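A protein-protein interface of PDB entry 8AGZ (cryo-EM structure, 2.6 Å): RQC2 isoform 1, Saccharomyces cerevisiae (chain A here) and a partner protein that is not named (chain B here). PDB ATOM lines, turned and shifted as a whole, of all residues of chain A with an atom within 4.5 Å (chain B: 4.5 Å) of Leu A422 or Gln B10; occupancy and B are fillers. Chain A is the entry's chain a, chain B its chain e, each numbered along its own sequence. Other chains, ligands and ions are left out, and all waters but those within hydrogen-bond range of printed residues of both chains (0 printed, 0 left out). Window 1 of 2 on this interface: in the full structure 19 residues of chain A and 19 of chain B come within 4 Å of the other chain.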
ATOM      1  N   LEU A 409      16.535  22.567 -26.133  1.00  0.00           N
ATOM      2  CA  LEU A 409      17.737  22.130 -25.421  1.00  0.00           C
ATOM      3  C   LEU A 409      18.716  21.403 -26.339  1.00  0.00           C
ATOM      4  O   LEU A 409      19.932  21.485 -26.137  1.00  0.00           O
ATOM      5  CB  LEU A 409      17.384  21.263 -24.212  1.00  0.00           C
ATOM      6  CG  LEU A 409      17.018  21.932 -22.880  1.00  0.00           C
ATOM      7  CD1 LEU A 409      18.246  22.673 -22.409  1.00  0.00           C
ATOM      8  CD2 LEU A 409      15.853  22.895 -22.907  1.00  0.00           C
ATOM      9  N   THR A 418      23.751  15.720 -19.454  1.00  0.00           N
ATOM     10  CA  THR A 418      23.416  16.970 -18.786  1.00  0.00           C
ATOM     11  C   THR A 418      21.973  17.380 -19.042  1.00  0.00           C
ATOM     12  O   THR A 418      21.337  17.952 -18.152  1.00  0.00           O
ATOM     13  CB  THR A 418      24.350  18.087 -19.244  1.00  0.00           C
ATOM     14  OG1 THR A 418      24.191  18.285 -20.650  1.00  0.00           O
ATOM     15  CG2 THR A 418      25.787  17.713 -18.971  1.00  0.00           C
ATOM     16  N   ILE A 419      21.435  17.066 -20.224  1.00  0.00           N
ATOM     17  CA  ILE A 419      20.018  17.307 -20.484  1.00  0.00           C
ATOM     18  C   ILE A 419      19.149  16.420 -19.598  1.00  0.00           C
ATOM     19  O   ILE A 419      18.161  16.895 -19.025  1.00  0.00           O
ATOM     20  CB  ILE A 419      19.709  17.107 -21.979  1.00  0.00           C
ATOM     21  CG1 ILE A 419      20.326  18.237 -22.803  1.00  0.00           C
ATOM     22  CG2 ILE A 419      18.213  17.046 -22.245  1.00  0.00           C
ATOM     23  CD1 ILE A 419      20.084  18.115 -24.295  1.00  0.00           C
ATOM     24  N   GLU A 420      19.526  15.149 -19.427  1.00  0.00           N
ATOM     25  CA  GLU A 420      18.770  14.263 -18.539  1.00  0.00           C
ATOM     26  C   GLU A 420      18.854  14.711 -17.082  1.00  0.00           C
ATOM     27  O   GLU A 420      17.868  14.610 -16.340  1.00  0.00           O
ATOM     28  CB  GLU A 420      19.256  12.823 -18.689  1.00  0.00           C
ATOM     29  CG  GLU A 420      18.852  12.172 -20.002  1.00  0.00           C
ATOM     30  CD  GLU A 420      19.719  10.983 -20.361  1.00  0.00           C
ATOM     31  OE1 GLU A 420      20.067  10.204 -19.451  1.00  0.00           O
ATOM     32  OE2 GLU A 420      20.039  10.818 -21.557  1.00  0.00           O
ATOM     33  N   LYS A 421      20.011  15.228 -16.659  1.00  0.00           N
ATOM     34  CA  LYS A 421      20.135  15.747 -15.299  1.00  0.00           C
ATOM     35  C   LYS A 421      19.302  17.011 -15.115  1.00  0.00           C
ATOM     36  O   LYS A 421      18.721  17.234 -14.042  1.00  0.00           O
ATOM     37  CB  LYS A 421      21.603  16.012 -14.969  1.00  0.00           C
ATOM     38  CG  LYS A 421      22.435  14.746 -14.852  1.00  0.00           C
ATOM     39  CD  LYS A 421      22.049  13.917 -13.641  1.00  0.00           C
ATOM     40  CE  LYS A 421      22.203  14.706 -12.357  1.00  0.00           C
ATOM     41  NZ  LYS A 421      23.629  15.055 -12.134  1.00  0.00           N
ATOM     42  N   LEU A 422      19.218  17.839 -16.158  1.00  0.00           N
ATOM     43  CA  LEU A 422      18.321  18.987 -16.143  1.00  0.00           C
ATOM     44  C   LEU A 422      16.858  18.575 -16.077  1.00  0.00           C
ATOM     45  O   LEU A 422      16.058  19.274 -15.446  1.00  0.00           O
ATOM     46  CB  LEU A 422      18.572  19.849 -17.379  1.00  0.00           C
ATOM     47  CG  LEU A 422      17.790  21.155 -17.495  1.00  0.00           C
ATOM     48  CD1 LEU A 422      18.057  22.034 -16.298  1.00  0.00           C
ATOM     49  CD2 LEU A 422      18.148  21.879 -18.766  1.00  0.00           C
ATOM     50  N   ILE A 423      16.492  17.459 -16.705  1.00  0.00           N
ATOM     51  CA  ILE A 423      15.120  16.969 -16.599  1.00  0.00           C
ATOM     52  C   ILE A 423      14.833  16.474 -15.185  1.00  0.00           C
ATOM     53  O   ILE A 423      13.770  16.764 -14.623  1.00  0.00           O
ATOM     54  CB  ILE A 423      14.845  15.882 -17.656  1.00  0.00           C
ATOM     55  CG1 ILE A 423      14.964  16.466 -19.060  1.00  0.00           C
ATOM     56  CG2 ILE A 423      13.450  15.300 -17.499  1.00  0.00           C
ATOM     57  CD1 ILE A 423      13.997  17.586 -19.336  1.00  0.00           C
ATOM     58  N   LYS A 424      15.790  15.754 -14.580  1.00  0.00           N
ATOM     59  CA  LYS A 424      15.617  15.267 -13.209  1.00  0.00           C
ATOM     60  C   LYS A 424      15.484  16.407 -12.208  1.00  0.00           C
ATOM     61  O   LYS A 424      14.631  16.359 -11.310  1.00  0.00           O
ATOM     62  CB  LYS A 424      16.783  14.368 -12.796  1.00  0.00           C
ATOM     63  CG  LYS A 424      16.920  13.102 -13.589  1.00  0.00           C
ATOM     64  CD  LYS A 424      17.992  12.193 -13.028  1.00  0.00           C
ATOM     65  CE  LYS A 424      18.291  11.059 -13.993  1.00  0.00           C
ATOM     66  NZ  LYS A 424      19.343  10.147 -13.472  1.00  0.00           N
ATOM     67  N   SER A 425      16.314  17.445 -12.352  1.00  0.00           N
ATOM     68  CA  SER A 425      16.262  18.563 -11.418  1.00  0.00           C
ATOM     69  C   SER A 425      14.963  19.346 -11.546  1.00  0.00           C
ATOM     70  O   SER A 425      14.382  19.761 -10.539  1.00  0.00           O
ATOM     71  CB  SER A 425      17.458  19.480 -11.635  1.00  0.00           C
ATOM     72  OG  SER A 425      17.254  20.739 -11.022  1.00  0.00           O
ATOM     73  N   GLU A 426      14.473  19.536 -12.770  1.00  0.00           N
ATOM     74  CA  GLU A 426      13.214  20.255 -12.934  1.00  0.00           C
ATOM     75  C   GLU A 426      12.015  19.410 -12.518  1.00  0.00           C
ATOM     76  O   GLU A 426      10.992  19.963 -12.097  1.00  0.00           O
ATOM     77  CB  GLU A 426      13.071  20.742 -14.374  1.00  0.00           C
ATOM     78  CG  GLU A 426      14.053  21.834 -14.759  1.00  0.00           C
ATOM     79  CD  GLU A 426      13.852  23.113 -13.965  1.00  0.00           C
ATOM     80  OE1 GLU A 426      12.692  23.432 -13.624  1.00  0.00           O
ATOM     81  OE2 GLU A 426      14.855  23.797 -13.673  1.00  0.00           O
ATOM     82  N   ASN B   7      16.409  28.659 -24.077  1.00  0.00           N
ATOM     83  CA  ASN B   7      16.234  28.028 -22.774  1.00  0.00           C
ATOM     84  C   ASN B   7      14.780  28.029 -22.336  1.00  0.00           C
ATOM     85  O   ASN B   7      14.417  28.739 -21.407  1.00  0.00           O
ATOM     86  CB  ASN B   7      17.091  28.740 -21.736  1.00  0.00           C
ATOM     87  CG  ASN B   7      18.511  28.216 -21.698  1.00  0.00           C
ATOM     88  OD1 ASN B   7      18.741  27.012 -21.781  1.00  0.00           O
ATOM     89  ND2 ASN B   7      19.472  29.120 -21.556  1.00  0.00           N
ATOM     90  N   THR B   8      13.953  27.226 -22.992  1.00  0.00           N
ATOM     91  CA  THR B   8      12.529  27.151 -22.658  1.00  0.00           C
ATOM     92  C   THR B   8      12.228  26.617 -21.265  1.00  0.00           C
ATOM     93  O   THR B   8      11.325  27.105 -20.596  1.00  0.00           O
ATOM     94  CB  THR B   8      11.762  26.304 -23.687  1.00  0.00           C
ATOM     95  OG1 THR B   8      12.540  25.150 -24.019  1.00  0.00           O
ATOM     96  CG2 THR B   8      11.507  27.103 -24.949  1.00  0.00           C
ATOM     97  N   PHE B   9      12.968  25.606 -20.832  1.00  0.00           N
ATOM     98  CA  PHE B   9      12.711  25.020 -19.528  1.00  0.00           C
ATOM     99  C   PHE B   9      12.914  26.025 -18.414  1.00  0.00           C
ATOM    100  O   PHE B   9      12.135  26.069 -17.467  1.00  0.00           O
ATOM    101  CB  PHE B   9      13.572  23.785 -19.294  1.00  0.00           C
ATOM    102  CG  PHE B   9      12.874  22.502 -19.617  1.00  0.00           C
ATOM    103  CD1 PHE B   9      11.882  22.021 -18.788  1.00  0.00           C
ATOM    104  CD2 PHE B   9      13.202  21.782 -20.747  1.00  0.00           C
ATOM    105  CE1 PHE B   9      11.230  20.843 -19.078  1.00  0.00           C
ATOM    106  CE2 PHE B   9      12.557  20.600 -21.044  1.00  0.00           C
ATOM    107  CZ  PHE B   9      11.566  20.130 -20.209  1.00  0.00           C
ATOM    108  N   GLN B  10      13.950  26.844 -18.530  1.00  0.00           N
ATOM    109  CA  GLN B  10      14.202  27.865 -17.524  1.00  0.00           C
ATOM    110  C   GLN B  10      13.035  28.837 -17.489  1.00  0.00           C
ATOM    111  O   GLN B  10      12.655  29.321 -16.424  1.00  0.00           O
ATOM    112  CB  GLN B  10      15.496  28.609 -17.825  1.00  0.00           C
ATOM    113  CG  GLN B  10      16.625  27.716 -18.317  1.00  0.00           C
ATOM    114  CD  GLN B  10      17.216  26.833 -17.236  1.00  0.00           C
ATOM    115  OE1 GLN B  10      17.127  27.138 -16.047  1.00  0.00           O
ATOM    116  NE2 GLN B  10      17.838  25.735 -17.648  1.00  0.00           N
ATOM    117  N   GLN B  11      12.481  29.148 -18.655  1.00  0.00           N
ATOM    118  CA  GLN B  11      11.347  30.054 -18.724  1.00  0.00           C
ATOM    119  C   GLN B  11      10.129  29.508 -18.003  1.00  0.00           C
ATOM    120  O   GLN B  11       9.388  30.258 -17.377  1.00  0.00           O
ATOM    121  CB  GLN B  11      11.002  30.363 -20.173  1.00  0.00           C
ATOM    122  CG  GLN B  11      12.113  31.089 -20.907  1.00  0.00           C
ATOM    123  CD  GLN B  11      11.999  30.956 -22.410  1.00  0.00           C
ATOM    124  OE1 GLN B  11      11.059  30.348 -22.921  1.00  0.00           O
ATOM    125  NE2 GLN B  11      12.962  31.522 -23.128  1.00  0.00           N
ATOM    126  N   TYR B  12       9.900  28.207 -18.105  1.00  0.00           N
ATOM    127  CA  TYR B  12       8.776  27.612 -17.402  1.00  0.00           C
ATOM    128  C   TYR B  12       8.974  27.785 -15.912  1.00  0.00           C
ATOM    129  O   TYR B  12       8.025  28.062 -15.183  1.00  0.00           O
ATOM    130  CB  TYR B  12       8.650  26.122 -17.706  1.00  0.00           C
ATOM    131  CG  TYR B  12       8.532  25.759 -19.166  1.00  0.00           C
ATOM    132  CD1 TYR B  12       7.703  26.470 -20.021  1.00  0.00           C
ATOM    133  CD2 TYR B  12       9.229  24.677 -19.682  1.00  0.00           C
ATOM    134  CE1 TYR B  12       7.592  26.127 -21.354  1.00  0.00           C
ATOM    135  CE2 TYR B  12       9.129  24.327 -21.013  1.00  0.00           C
ATOM    136  CZ  TYR B  12       8.306  25.053 -21.844  1.00  0.00           C
ATOM    137  OH  TYR B  12       8.201  24.701 -23.171  1.00  0.00           O
ATOM    138  N   ASN B  13      10.207  27.614 -15.454  1.00  0.00           N
ATOM    139  CA  ASN B  13      10.510  27.730 -14.029  1.00  0.00           C
ATOM    140  C   ASN B  13      10.256  29.120 -13.451  1.00  0.00           C
ATOM    141  O   ASN B  13       9.765  29.229 -12.330  1.00  0.00           O
ATOM    142  CB  ASN B  13      11.966  27.310 -13.777  1.00  0.00           C
ATOM    143  CG  ASN B  13      12.378  27.462 -12.325  1.00  0.00           C
ATOM    144  OD1 ASN B  13      11.747  26.906 -11.426  1.00  0.00           O
ATOM    145  ND2 ASN B  13      13.448  28.211 -12.091  1.00  0.00           N
ATOM    146  N   THR B  14      10.604  30.173 -14.189  1.00  0.00           N
ATOM    147  CA  THR B  14      10.463  31.547 -13.686  1.00  0.00           C
ATOM    148  C   THR B  14      11.194  31.750 -12.357  1.00  0.00           C
ATOM    149  O   THR B  14      10.700  32.451 -11.475  1.00  0.00           O
ATOM    150  CB  THR B  14       8.996  32.031 -13.561  1.00  0.00           C
ATOM    151  OG1 THR B  14       8.390  31.486 -12.383  1.00  0.00           O
ATOM    152  CG2 THR B  14       8.177  31.658 -14.784  1.00  0.00           C
ATOM    153  N   ARG B  24      18.644  33.547 -14.287  1.00  0.00           N
ATOM    154  CA  ARG B  24      18.864  32.513 -13.301  1.00  0.00           C
ATOM    155  C   ARG B  24      20.347  32.312 -13.135  1.00  0.00           C
ATOM    156  O   ARG B  24      21.062  32.126 -14.113  1.00  0.00           O
ATOM    157  CB  ARG B  24      18.217  31.210 -13.737  1.00  0.00           C
ATOM    158  CG  ARG B  24      18.562  30.031 -12.847  1.00  0.00           C
ATOM    159  CD  ARG B  24      17.589  28.882 -13.028  1.00  0.00           C
ATOM    160  NE  ARG B  24      17.987  27.725 -12.232  1.00  0.00           N
ATOM    161  CZ  ARG B  24      17.660  27.545 -10.956  1.00  0.00           C
ATOM    162  NH1 ARG B  24      16.924  28.445 -10.320  1.00  0.00           N
ATOM    163  NH2 ARG B  24      18.076  26.464 -10.317  1.00  0.00           N
ATOM    164  N   PHE B  30      24.116  21.792 -14.788  1.00  0.00           N
ATOM    165  CA  PHE B  30      23.064  21.678 -15.791  1.00  0.00           C
ATOM    166  C   PHE B  30      22.341  22.964 -16.167  1.00  0.00           C
ATOM    167  O   PHE B  30      22.001  23.152 -17.325  1.00  0.00           O
ATOM    168  CB  PHE B  30      22.066  20.556 -15.478  1.00  0.00           C
ATOM    169  CG  PHE B  30      21.894  20.270 -14.024  1.00  0.00           C
ATOM    170  CD1 PHE B  30      20.966  20.963 -13.281  1.00  0.00           C
ATOM    171  CD2 PHE B  30      22.633  19.277 -13.412  1.00  0.00           C
ATOM    172  CE1 PHE B  30      20.795  20.694 -11.943  1.00  0.00           C
ATOM    173  CE2 PHE B  30      22.469  18.999 -12.075  1.00  0.00           C
ATOM    174  CZ  PHE B  30      21.544  19.709 -11.340  1.00  0.00           C
ATOM    175  N   ASP B  31      22.093  23.848 -15.214  1.00  0.00           N
ATOM    176  CA  ASP B  31      21.306  25.041 -15.520  1.00  0.00           C
ATOM    177  C   ASP B  31      21.969  26.353 -15.164  1.00  0.00           C
ATOM    178  O   ASP B  31      22.941  26.378 -14.424  1.00  0.00           O
ATOM    179  CB  ASP B  31      19.924  24.966 -14.874  1.00  0.00           C
ATOM    180  CG  ASP B  31      19.979  24.948 -13.359  1.00  0.00           C
ATOM    181  OD1 ASP B  31      20.180  26.015 -12.746  1.00  0.00           O
ATOM    182  OD2 ASP B  31      19.795  23.863 -12.777  1.00  0.00           O
ATOM    183  N   GLY B  32      21.439  27.445 -15.693  1.00  0.00           N
ATOM    184  CA  GLY B  32      22.019  28.753 -15.442  1.00  0.00           C
ATOM    185  C   GLY B  32      23.024  29.128 -16.500  1.00  0.00           C
ATOM    186  O   GLY B  32      23.649  30.185 -16.424  1.00  0.00           O
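Of the printed residues of chain B, Leu A409 touches Phe B9 (3.6 Å). Printed residues of chain B within 4 Å of Thr A418: Phe B30 (3.8 Å). Of the printed residues of chain B, Lys A421 touches Phe B30 (3.8 Å). Of the printed residues of chain B, Leu A422 touches Gln B10 (3.9 Å), Phe B30 (3.99 Å) and Asp B31 (3.8 Å). Of the printed residues of chain B, Ile A423 touches Phe B9. Of the printed residues of chain A, Gln B10 touches Leu A422 (3.9 Å). Of the printed residues of chain A, Asn B13 touches Glu A426 (3.9 Å). The nearest printed residue of chain B that does not touch Leu A422 is Phe B9 (5.0 Å). The nearest printed residue of chain A that does not touch Gln B10 is Glu A426 (4.7 Å).
Hydrophobic or aromatic side chains of chain B that line the printed part of chain A: Phe B9 and Phe B30. Among the printed residues, 9 pairs touch across the chains. Among the printed residues, no Asp or Glu carboxylate lies within 4 Å of a Lys or Arg side-chain nitrogen of the other chain.
OD1 of Asp B31 is in salt-bridge range of NE of Arg B24.
Leu A409 touches Phe B9. O of Thr A418 touches CB of Phe B30, at 3.8 Å. Phe B30 touches Lys A421. Leu A422 touches Gln B10. Leu A422 touches Phe B30. Leu A422 touches Asp B31 (CD1 to CB, 3.8 Å). CD1 of Ile A423 touches CZ of Phe B9, at 3.6 Å. CB of Ser A425 touches CE1 of Phe B30 (3.6 Å). Asn B13 touches Glu A426.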
